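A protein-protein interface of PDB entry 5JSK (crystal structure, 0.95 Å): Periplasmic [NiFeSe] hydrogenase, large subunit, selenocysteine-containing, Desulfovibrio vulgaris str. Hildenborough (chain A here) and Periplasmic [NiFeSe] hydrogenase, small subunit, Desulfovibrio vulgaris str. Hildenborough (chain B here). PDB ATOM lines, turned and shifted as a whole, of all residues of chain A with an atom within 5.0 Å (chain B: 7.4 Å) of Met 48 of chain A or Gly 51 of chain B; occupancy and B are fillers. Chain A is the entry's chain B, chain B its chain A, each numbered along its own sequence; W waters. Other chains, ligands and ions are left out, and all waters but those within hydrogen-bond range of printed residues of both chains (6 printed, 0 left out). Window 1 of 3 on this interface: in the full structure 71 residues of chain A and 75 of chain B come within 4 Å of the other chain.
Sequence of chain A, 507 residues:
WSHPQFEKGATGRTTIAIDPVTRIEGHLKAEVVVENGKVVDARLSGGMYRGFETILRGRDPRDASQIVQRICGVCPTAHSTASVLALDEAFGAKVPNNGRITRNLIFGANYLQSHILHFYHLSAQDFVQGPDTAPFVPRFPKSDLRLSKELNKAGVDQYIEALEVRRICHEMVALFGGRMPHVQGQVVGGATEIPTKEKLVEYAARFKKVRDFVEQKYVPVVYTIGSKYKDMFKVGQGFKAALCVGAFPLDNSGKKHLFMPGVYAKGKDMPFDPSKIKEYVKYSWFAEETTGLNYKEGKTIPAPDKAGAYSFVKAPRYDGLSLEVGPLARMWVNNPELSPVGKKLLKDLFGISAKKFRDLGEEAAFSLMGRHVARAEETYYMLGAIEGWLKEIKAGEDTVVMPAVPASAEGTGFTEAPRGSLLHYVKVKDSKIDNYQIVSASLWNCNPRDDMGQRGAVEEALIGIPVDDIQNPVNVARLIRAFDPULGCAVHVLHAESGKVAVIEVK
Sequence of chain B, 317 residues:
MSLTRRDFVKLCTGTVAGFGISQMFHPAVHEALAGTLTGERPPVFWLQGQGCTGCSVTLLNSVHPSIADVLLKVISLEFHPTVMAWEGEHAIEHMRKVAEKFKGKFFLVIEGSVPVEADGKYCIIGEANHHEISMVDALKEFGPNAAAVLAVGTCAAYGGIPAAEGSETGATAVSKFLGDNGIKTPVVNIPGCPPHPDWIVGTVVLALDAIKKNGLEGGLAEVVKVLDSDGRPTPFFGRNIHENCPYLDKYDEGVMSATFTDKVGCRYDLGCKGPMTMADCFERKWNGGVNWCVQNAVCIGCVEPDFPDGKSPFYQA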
ATOM      1  N   GLU A  25      -6.626   4.778   3.552  1.00  0.00           N
ATOM      2  CA  GLU A  25      -5.486   5.260   2.782  1.00  0.00           C
ATOM      3  C   GLU A  25      -4.949   4.140   1.903  1.00  0.00           C
ATOM      4  O   GLU A  25      -4.740   3.013   2.366  1.00  0.00           O
ATOM      5  CB  GLU A  25      -4.375   5.822   3.674  1.00  0.00           C
ATOM      6  CG  GLU A  25      -3.260   6.575   2.931  1.00  0.00           C
ATOM      7  CD  GLU A  25      -2.383   5.720   2.017  1.00  0.00           C
ATOM      8  OE1 GLU A  25      -2.158   4.529   2.308  1.00  0.00           O
ATOM      9  OE2 GLU A  25      -1.921   6.256   0.970  1.00  0.00           O
ATOM     10  N   HIS A  27      -4.110   1.610  -1.573  1.00  0.00           N
ATOM     11  CA  HIS A  27      -4.671   0.667  -2.535  1.00  0.00           C
ATOM     12  C   HIS A  27      -4.877  -0.700  -1.897  1.00  0.00           C
ATOM     13  O   HIS A  27      -3.904  -1.413  -1.615  1.00  0.00           O
ATOM     14  CB  HIS A  27      -3.740   0.547  -3.737  1.00  0.00           C
ATOM     15  CG  HIS A  27      -3.642   1.803  -4.544  1.00  0.00           C
ATOM     16  ND1 HIS A  27      -4.703   2.301  -5.265  1.00  0.00           N
ATOM     17  CD2 HIS A  27      -2.602   2.642  -4.773  1.00  0.00           C
ATOM     18  CE1 HIS A  27      -4.320   3.399  -5.894  1.00  0.00           C
ATOM     19  NE2 HIS A  27      -3.048   3.627  -5.619  1.00  0.00           N
ATOM     20  N   GLY A  46      -2.715  -5.777  -1.019  1.00  0.00           N
ATOM     21  CA  GLY A  46      -2.166  -4.450  -1.205  1.00  0.00           C
ATOM     22  C   GLY A  46      -1.565  -4.376  -2.589  1.00  0.00           C
ATOM     23  O   GLY A  46      -0.578  -5.056  -2.882  1.00  0.00           O
ATOM     24  N   GLY A  47      -2.189  -3.586  -3.459  1.00  0.00           N
ATOM     25  CA  GLY A  47      -1.897  -3.605  -4.871  1.00  0.00           C
ATOM     26  C   GLY A  47      -0.940  -2.566  -5.403  1.00  0.00           C
ATOM     27  O   GLY A  47      -0.794  -2.484  -6.630  1.00  0.00           O
ATOM     28  N   MET A  48      -0.269  -1.790  -4.546  1.00  0.00           N
ATOM     29  CA  MET A  48       0.666  -0.778  -5.018  1.00  0.00           C
ATOM     30  C   MET A  48       1.967  -0.865  -4.243  1.00  0.00           C
ATOM     31  O   MET A  48       1.957  -0.963  -3.013  1.00  0.00           O
ATOM     32  CB  MET A  48       0.054   0.625  -4.941  1.00  0.00           C
ATOM     33  CG  MET A  48       0.947   1.727  -5.545  1.00  0.00           C
ATOM     34  SD  MET A  48       2.214   2.382  -4.434  1.00  0.00           S
ATOM     35  CE  MET A  48       1.230   3.461  -3.396  1.00  0.00           C
ATOM     36  N   TYR A  49       3.081  -0.828  -4.973  1.00  0.00           N
ATOM     37  CA  TYR A  49       4.414  -0.925  -4.398  1.00  0.00           C
ATOM     38  C   TYR A  49       5.285   0.216  -4.898  1.00  0.00           C
ATOM     39  O   TYR A  49       5.247   0.559  -6.083  1.00  0.00           O
ATOM     40  CB  TYR A  49       5.042  -2.266  -4.812  1.00  0.00           C
ATOM     41  CG  TYR A  49       6.479  -2.484  -4.415  1.00  0.00           C
ATOM     42  CD1 TYR A  49       6.823  -2.927  -3.150  1.00  0.00           C
ATOM     43  CD2 TYR A  49       7.507  -2.269  -5.328  1.00  0.00           C
ATOM     44  CE1 TYR A  49       8.143  -3.147  -2.798  1.00  0.00           C
ATOM     45  CE2 TYR A  49       8.832  -2.484  -4.986  1.00  0.00           C
ATOM     46  CZ  TYR A  49       9.152  -2.926  -3.722  1.00  0.00           C
ATOM     47  OH  TYR A  49      10.441  -3.163  -3.329  1.00  0.00           O
ATOM     48  N   ARG A  50       6.112   0.750  -3.998  1.00  0.00           N
ATOM     49  CA  ARG A  50       7.138   1.736  -4.330  1.00  0.00           C
ATOM     50  C   ARG A  50       8.552   1.273  -4.025  1.00  0.00           C
ATOM     51  O   ARG A  50       9.453   1.566  -4.807  1.00  0.00           O
ATOM     52  CB  ARG A  50       6.834   3.080  -3.629  1.00  0.00           C
ATOM     53  CG  ARG A  50       5.647   3.780  -4.273  1.00  0.00           C
ATOM     54  CD  ARG A  50       5.035   4.897  -3.445  1.00  0.00           C
ATOM     55  NE  ARG A  50       4.488   4.365  -2.211  1.00  0.00           N
ATOM     56  CZ  ARG A  50       4.272   5.068  -1.103  1.00  0.00           C
ATOM     57  NH1 ARG A  50       4.435   6.384  -1.103  1.00  0.00           N
ATOM     58  NH2 ARG A  50       3.920   4.440   0.014  1.00  0.00           N
ATOM     59  N   PHE A 312       1.438  -7.046  -2.066  1.00  0.00           N
ATOM     60  CA  PHE A 312       2.760  -6.462  -1.853  1.00  0.00           C
ATOM     61  C   PHE A 312       3.063  -6.226  -0.380  1.00  0.00           C
ATOM     62  O   PHE A 312       4.150  -5.741  -0.047  1.00  0.00           O
ATOM     63  CB  PHE A 312       2.935  -5.154  -2.633  1.00  0.00           C
ATOM     64  CG  PHE A 312       3.061  -5.322  -4.122  1.00  0.00           C
ATOM     65  CD1 PHE A 312       4.171  -5.939  -4.678  1.00  0.00           C
ATOM     66  CD2 PHE A 312       2.083  -4.823  -4.972  1.00  0.00           C
ATOM     67  CE1 PHE A 312       4.289  -6.069  -6.050  1.00  0.00           C
ATOM     68  CE2 PHE A 312       2.204  -4.945  -6.354  1.00  0.00           C
ATOM     69  CZ  PHE A 312       3.295  -5.580  -6.887  1.00  0.00           C
ATOM     70  N   VAL A 491       2.853  -1.399   2.601  1.00  0.00           N
ATOM     71  CA  VAL A 491       3.732  -1.879   1.533  1.00  0.00           C
ATOM     72  C   VAL A 491       5.054  -1.127   1.485  1.00  0.00           C
ATOM     73  O   VAL A 491       6.113  -1.733   1.279  1.00  0.00           O
ATOM     74  CB  VAL A 491       3.039  -1.794   0.160  1.00  0.00           C
ATOM     75  CG1 VAL A 491       4.011  -2.254  -0.919  1.00  0.00           C
ATOM     76  CG2 VAL A 491       1.762  -2.596   0.112  1.00  0.00           C
ATOM     77  N   GLN B  48      -5.279   8.017  -7.722  1.00  0.00           N
ATOM     78  CA  GLN B  48      -4.025   7.821  -7.015  1.00  0.00           C
ATOM     79  C   GLN B  48      -3.255   6.685  -7.668  1.00  0.00           C
ATOM     80  O   GLN B  48      -3.765   5.563  -7.781  1.00  0.00           O
ATOM     81  CB  GLN B  48      -4.292   7.524  -5.539  1.00  0.00           C
ATOM     82  CG  GLN B  48      -4.869   8.732  -4.843  1.00  0.00           C
ATOM     83  CD  GLN B  48      -5.399   8.492  -3.449  1.00  0.00           C
ATOM     84  OE1 GLN B  48      -5.798   7.385  -3.087  1.00  0.00           O
ATOM     85  NE2 GLN B  48      -5.456   9.555  -2.660  1.00  0.00           N
ATOM     86  N   GLY B  49      -2.030   6.981  -8.087  1.00  0.00           N
ATOM     87  CA  GLY B  49      -1.091   5.977  -8.533  1.00  0.00           C
ATOM     88  C   GLY B  49      -0.166   5.604  -7.396  1.00  0.00           C
ATOM     89  O   GLY B  49      -0.628   5.208  -6.327  1.00  0.00           O
ATOM     90  N   GLN B  50       1.140   5.780  -7.595  1.00  0.00           N
ATOM     91  CA  GLN B  50       2.129   5.553  -6.537  1.00  0.00           C
ATOM     92  C   GLN B  50       2.255   6.814  -5.686  1.00  0.00           C
ATOM     93  O   GLN B  50       3.262   7.517  -5.713  1.00  0.00           O
ATOM     94  CB  GLN B  50       3.472   5.180  -7.136  1.00  0.00           C
ATOM     95  CG  GLN B  50       3.478   3.841  -7.832  1.00  0.00           C
ATOM     96  CD  GLN B  50       4.768   3.641  -8.591  1.00  0.00           C
ATOM     97  OE1 GLN B  50       5.078   4.407  -9.508  1.00  0.00           O
ATOM     98  NE2 GLN B  50       5.547   2.635  -8.202  1.00  0.00           N
ATOM     99  N   GLY B  51       1.175   7.103  -4.960  1.00  0.00           N
ATOM    100  CA  GLY B  51       1.086   8.262  -4.103  1.00  0.00           C
ATOM    101  C   GLY B  51       1.126   7.835  -2.643  1.00  0.00           C
ATOM    102  O   GLY B  51       1.005   6.654  -2.302  1.00  0.00           O
ATOM    103  N   CYS B  52       1.305   8.835  -1.775  1.00  0.00           N
ATOM    104  CA  CYS B  52       1.305   8.638  -0.334  1.00  0.00           C
ATOM    105  C   CYS B  52       0.070   9.225   0.331  1.00  0.00           C
ATOM    106  O   CYS B  52      -0.052   9.171   1.563  1.00  0.00           O
ATOM    107  CB  CYS B  52       2.564   9.238   0.301  1.00  0.00           C
ATOM    108  SG  CYS B  52       2.519  11.063   0.486  1.00  0.00           S
ATOM    109  N   THR B  53      -0.835   9.819  -0.454  1.00  0.00           N
ATOM    110  CA  THR B  53      -2.041  10.501   0.007  1.00  0.00           C
ATOM    111  C   THR B  53      -1.721  11.874   0.604  1.00  0.00           C
ATOM    112  O   THR B  53      -2.641  12.615   0.973  1.00  0.00           O
ATOM    113  CB  THR B  53      -2.917   9.579   0.870  1.00  0.00           C
ATOM    114  OG1 THR B  53      -3.136   8.392   0.096  1.00  0.00           O
ATOM    115  CG2 THR B  53      -4.275  10.166   1.201  1.00  0.00           C
ATOM    116  N   GLY B  54      -0.450  12.269   0.626  1.00  0.00           N
ATOM    117  CA  GLY B  54      -0.078  13.574   1.142  1.00  0.00           C
ATOM    118  C   GLY B  54      -0.556  14.731   0.292  1.00  0.00           C
ATOM    119  O   GLY B  54      -0.747  15.836   0.804  1.00  0.00           O
ATOM    120  N   CYS B  55      -0.697  14.514  -1.017  1.00  0.00           N
ATOM    121  CA  CYS B  55      -1.240  15.552  -1.882  1.00  0.00           C
ATOM    122  C   CYS B  55      -2.733  15.750  -1.613  1.00  0.00           C
ATOM    123  O   CYS B  55      -3.233  16.878  -1.636  1.00  0.00           O
ATOM    124  CB  CYS B  55      -0.946  15.228  -3.346  1.00  0.00           C
ATOM    125  SG  CYS B  55       0.798  15.463  -3.832  1.00  0.00           S
ATOM    126  N   GLU B 111      -2.452  11.914  -8.495  1.00  0.00           N
ATOM    127  CA  GLU B 111      -1.584  11.960  -7.322  1.00  0.00           C
ATOM    128  C   GLU B 111      -0.739  10.694  -7.350  1.00  0.00           C
ATOM    129  O   GLU B 111      -1.288   9.590  -7.415  1.00  0.00           O
ATOM    130  CB  GLU B 111      -2.447  12.008  -6.048  1.00  0.00           C
ATOM    131  CG  GLU B 111      -1.712  11.796  -4.732  1.00  0.00           C
ATOM    132  CD  GLU B 111      -2.584  11.998  -3.506  1.00  0.00           C
ATOM    133  OE1 GLU B 111      -3.835  11.876  -3.611  1.00  0.00           O
ATOM    134  OE2 GLU B 111      -2.025  12.290  -2.417  1.00  0.00           O
ATOM    135  N   GLY B 112       0.579  10.835  -7.305  1.00  0.00           N
ATOM    136  CA  GLY B 112       1.482   9.710  -7.424  1.00  0.00           C
ATOM    137  C   GLY B 112       1.962   9.503  -8.851  1.00  0.00           C
ATOM    138  O   GLY B 112       1.386  10.005  -9.810  1.00  0.00           O
ATOM    139  N   SER B 113       3.037   8.719  -8.980  1.00  0.00           N
ATOM    140  CA  SER B 113       3.591   8.363 -10.276  1.00  0.00           C
ATOM    141  C   SER B 113       2.867   7.148 -10.878  1.00  0.00           C
ATOM    142  O   SER B 113       2.053   6.482 -10.232  1.00  0.00           O
ATOM    143  CB  SER B 113       5.088   8.119 -10.149  1.00  0.00           C
ATOM    144  OG  SER B 113       5.366   7.163  -9.138  1.00  0.00           O
ATOM    145  N   PRO B 115       3.607   3.560 -12.587  1.00  0.00           N
ATOM    146  CA  PRO B 115       4.687   2.594 -12.818  1.00  0.00           C
ATOM    147  C   PRO B 115       4.392   1.709 -14.012  1.00  0.00           C
ATOM    148  O   PRO B 115       3.341   1.057 -14.073  1.00  0.00           O
ATOM    149  CB  PRO B 115       4.730   1.798 -11.511  1.00  0.00           C
ATOM    150  CG  PRO B 115       3.289   1.811 -11.025  1.00  0.00           C
ATOM    151  CD  PRO B 115       2.695   3.128 -11.514  1.00  0.00           C
ATOM    152  N   LYS B 121       1.765  -3.885 -13.075  1.00  0.00           N
ATOM    153  CA  LYS B 121       1.345  -4.606 -11.880  1.00  0.00           C
ATOM    154  C   LYS B 121       1.781  -3.956 -10.574  1.00  0.00           C
ATOM    155  O   LYS B 121       1.283  -4.358  -9.520  1.00  0.00           O
ATOM    156  CB  LYS B 121       1.884  -6.042 -11.930  1.00  0.00           C
ATOM    157  CG  LYS B 121       1.167  -6.966 -12.872  1.00  0.00           C
ATOM    158  CD  LYS B 121       1.710  -8.395 -12.724  1.00  0.00           C
ATOM    159  CE  LYS B 121       0.999  -9.377 -13.629  1.00  0.00           C
ATOM    160  NZ  LYS B 121       1.533 -10.751 -13.443  1.00  0.00           N
ATOM    161  N   TYR B 122       2.699  -2.986 -10.595  1.00  0.00           N
ATOM    162  CA  TYR B 122       3.093  -2.326  -9.356  1.00  0.00           C
ATOM    163  C   TYR B 122       2.068  -1.291  -8.890  1.00  0.00           C
ATOM    164  O   TYR B 122       2.254  -0.691  -7.831  1.00  0.00           O
ATOM    165  CB  TYR B 122       4.485  -1.712  -9.463  1.00  0.00           C
ATOM    166  CG  TYR B 122       5.603  -2.719  -9.542  1.00  0.00           C
ATOM    167  CD1 TYR B 122       5.855  -3.566  -8.483  1.00  0.00           C
ATOM    168  CD2 TYR B 122       6.434  -2.793 -10.649  1.00  0.00           C
ATOM    169  CE1 TYR B 122       6.896  -4.466  -8.513  1.00  0.00           C
ATOM    170  CE2 TYR B 122       7.491  -3.703 -10.698  1.00  0.00           C
ATOM    171  CZ  TYR B 122       7.720  -4.536  -9.613  1.00  0.00           C
ATOM    172  OH  TYR B 122       8.747  -5.449  -9.584  1.00  0.00           O
ATOM    173  N   CYS B 123       0.979  -1.077  -9.629  1.00  0.00           N
ATOM    174  CA  CYS B 123      -0.099  -0.227  -9.117  1.00  0.00           C
ATOM    175  C   CYS B 123      -1.428  -0.651  -9.731  1.00  0.00           C
ATOM    176  O   CYS B 123      -1.757  -0.255 -10.853  1.00  0.00           O
ATOM    177  CB  CYS B 123       0.177   1.240  -9.369  1.00  0.00           C
ATOM    178  SG  CYS B 123      -1.031   2.307  -8.540  1.00  0.00           S
ATOM    179  N   ILE B 124      -2.188  -1.446  -8.982  1.00  0.00           N
ATOM    180  CA  ILE B 124      -3.548  -1.826  -9.349  1.00  0.00           C
ATOM    181  C   ILE B 124      -4.507  -0.935  -8.572  1.00  0.00           C
ATOM    182  O   ILE B 124      -4.453  -0.879  -7.337  1.00  0.00           O
ATOM    183  CB  ILE B 124      -3.811  -3.310  -9.061  1.00  0.00           C
ATOM    184  CG1 ILE B 124      -2.830  -4.190  -9.852  1.00  0.00           C
ATOM    185  CG2 ILE B 124      -5.255  -3.668  -9.371  1.00  0.00           C
ATOM    186  CD1 ILE B 124      -2.847  -4.004 -11.354  1.00  0.00           C
ATOM    187  N   ILE B 125      -5.381  -0.220  -9.294  1.00  0.00           N
ATOM    188  CA  ILE B 125      -6.254   0.770  -8.669  1.00  0.00           C
ATOM    189  C   ILE B 125      -7.698   0.310  -8.519  1.00  0.00           C
ATOM    190  O   ILE B 125      -8.485   0.998  -7.860  1.00  0.00           O
ATOM    191  CB  ILE B 125      -6.191   2.148  -9.367  1.00  0.00           C
ATOM    192  CG1 ILE B 125      -6.938   2.168 -10.698  1.00  0.00           C
ATOM    193  CG2 ILE B 125      -4.746   2.576  -9.556  1.00  0.00           C
ATOM    194  CD1 ILE B 125      -7.238   3.557 -11.178  1.00  0.00           C
ATOM    195  N   CYS B 155       5.581  13.639  -7.412  1.00  0.00           N
ATOM    196  CA  CYS B 155       5.529  12.290  -7.983  1.00  0.00           C
ATOM    197  C   CYS B 155       4.837  12.308  -9.340  1.00  0.00           C
ATOM    198  O   CYS B 155       5.366  11.793 -10.338  1.00  0.00           O
ATOM    199  CB  CYS B 155       4.785  11.306  -7.083  1.00  0.00           C
ATOM    200  SG  CYS B 155       5.496  10.986  -5.464  1.00  0.00           S
ATOM    201  N   PRO B 162       9.247   7.891  -5.926  1.00  0.00           N
ATOM    202  CA  PRO B 162       9.121   6.545  -6.514  1.00  0.00           C
ATOM    203  C   PRO B 162      10.018   6.302  -7.717  1.00  0.00           C
ATOM    204  O   PRO B 162      10.277   5.138  -8.051  1.00  0.00           O
ATOM    205  CB  PRO B 162       7.635   6.458  -6.878  1.00  0.00           C
ATOM    206  CG  PRO B 162       6.977   7.361  -5.878  1.00  0.00           C
ATOM    207  CD  PRO B 162       7.923   8.540  -5.767  1.00  0.00           C
HETATM  208  O   HOH W   1       4.742   8.259  -3.237  1.00  0.00           O
HETATM  209  O   HOH W   2      -2.147   5.655  -3.330  1.00  0.00           O
HETATM  210  O   HOH W   3      -4.979   4.797  -3.262  1.00  0.00           O
HETATM  211  O   HOH W   4       9.098   2.783  -7.279  1.00  0.00           O
HETATM  212  O   HOH W   5      -0.707   4.881  -0.956  1.00  0.00           O
HETATM  213  O   HOH W   6      -6.984   0.865  -5.010  1.00  0.00           O
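Among the printed residues, pairs that only touch across the chains: Glu 25 of chain A with Cys 52 of chain B (3.5 Å), His 27 of chain A with Ile 124 of chain B (3.8 Å), His 27 of chain A with Ile 125 of chain B (3.8 Å), Gly 47 of chain A with Tyr 122 of chain B (3.7 Å), Gly 47 of chain A with Cys 123 of chain B (3.4 Å), Met 48 of chain A with Gly 49 of chain B (3.9 Å), Met 48 of chain A with Gln 50 of chain B (3.8 Å), Met 48 of chain A with Gly 51 of chain B (3.4 Å), Met 48 of chain A with Tyr 122 of chain B (3.2 Å), Met 48 of chain A with Cys 123 of chain B (3.6 Å), Arg 50 of chain A with Gln 50 of chain B (3.9 Å), Arg 50 of chain A with Gly 51 of chain B (3.6 Å), Arg 50 of chain A with Cys 52 of chain B (3.7 Å), Arg 50 of chain A with Pro 162 of chain B (3.97 Å), Phe 312 of chain A with Lys 121 of chain B (3.3 Å) and Phe 312 of chain A with Tyr 122 of chain B (3.6 Å).
Of chain B, only Gly 49, Gln 50, Gly 51, Tyr 122 and Cys 123 come within 4 Å of Met 48 of chain A. Of chain A, only Met 48 (3.4 Å) and Arg 50 (3.6 Å) come within 4 Å of Gly 51 of chain B. Gly 47 of chain A touches three residues of chain B. Printed residues of chain B within 4 Å of His 27 of chain A: Gln 48 (2.9 Å), Gly 49 (3.0 Å), Cys 123 (3.8 Å), Ile 124 (3.8 Å) and Ile 125 (3.8 Å). Of the printed residues of chain A, Gly 49 of chain B touches His 27 (3.0 Å) and Met 48 (3.9 Å). Of the printed residues of chain A, Ile 125 of chain B touches His 27. The nearest printed residue of chain B that does not touch Tyr 49 of chain A is Cys 123 of chain B (5.1 Å).
Water W5 bridges the side-chain carboxylate (OE2) of Glu 25 of chain A and the backbone carbonyl oxygen (O) of Gly 51 of chain B. Water W6 bridges a ring nitrogen (ND1) of His 27 of chain A (2.7 Å) and the backbone carbonyl oxygen (O) of Ile 125 of chain B (3.2 Å). Water W3 lies within hydrogen-bond range of the side-chain amide oxygen of Gln 48 of chain B and a ring nitrogen (ND1) of His 27 of chain A. Water W4 bridges the backbone carbonyl oxygen (O) of Pro 162 of chain B (2.7 Å) and the backbone carbonyl oxygen (O) of Arg 50 of chain A (2.8 Å). Water W1 bridges the guanidinium group of Arg 50 of chain A and the backbone carbonyl oxygen of Gln 50 of chain B. Water W2 lies within hydrogen-bond range of NE2 of His 27 of chain A, O of Gly 49 of chain B and O of Gly 51 of chain B.
Of the 19 printed residues of chain B, 12 touch a printed residue of chain A. Printed residues of chain B that touch a printed residue of chain A: Gln 48, Gly 49, Gln 50, Gly 51, Cys 52, Thr 53, Lys 121, Tyr 122, Cys 123, Ile 124, Ile 125 and Pro 162. Of the 9 printed residues of chain A, 7 touch a printed residue of chain B. Among the printed residues, no Asp or Glu carboxylate lies within 4 Å of a Lys or Arg side-chain nitrogen of the other chain.
The side-chain hydroxyl (OG1) of Thr 53 of chain B is in hydrogen-bond range of the side-chain carboxylate (OE2) of Glu 25 of chain A (2.6 Å). SG of Cys 123 of chain B is in hydrogen-bond range of NE2 of His 27 of chain A (3.8 Å). The backbone carbonyl oxygen (O) of Tyr 122 of chain B sits at hydrogen-bond distance from the backbone NH (N) of Tyr 49 of chain A. The backbone NH (N) of Ile 124 of chain B is in hydrogen-bond range of the backbone carbonyl oxygen (O) of Gly 47 of chain A, at 2.9 Å. A ring nitrogen (NE2) of His 27 of chain A is in hydrogen-bond range of the backbone carbonyl oxygen of Gly 49 of chain B (3.0 Å). A ring nitrogen (NE2) of His 27 of chain A lies close to the backbone carbonyl oxygen of Gln 48 of chain B, 3.0 Å away. The backbone carbonyl oxygen (O) of Tyr 49 of chain A sits at hydrogen-bond distance from the side-chain amide nitrogen (NE2) of Gln 50 of chain B, at 3.0 Å.
The backbone NH (N) of Gly 54 of chain B lies close to the side-chain sulfur (SG) of Cys 52 of chain B (3.2 Å). The side-chain carboxylate (OE2) of Glu 111 of chain B lies close to the backbone NH (N) of Thr 53 of chain B. O of His 27 of chain A sits at hydrogen-bond distance from N of Gly 47 of chain A (3.3 Å). O of Glu 111 of chain B sits at hydrogen-bond distance from N of Gly 49 of chain B, 2.8 Å away. SG of Cys 123 of chain B lies close to O of Gly 49 of chain B. The side-chain sulfur (SD) of Met 48 of chain A lies close to the guanidinium group (NE) of Arg 50 of chain A (3.7 Å).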
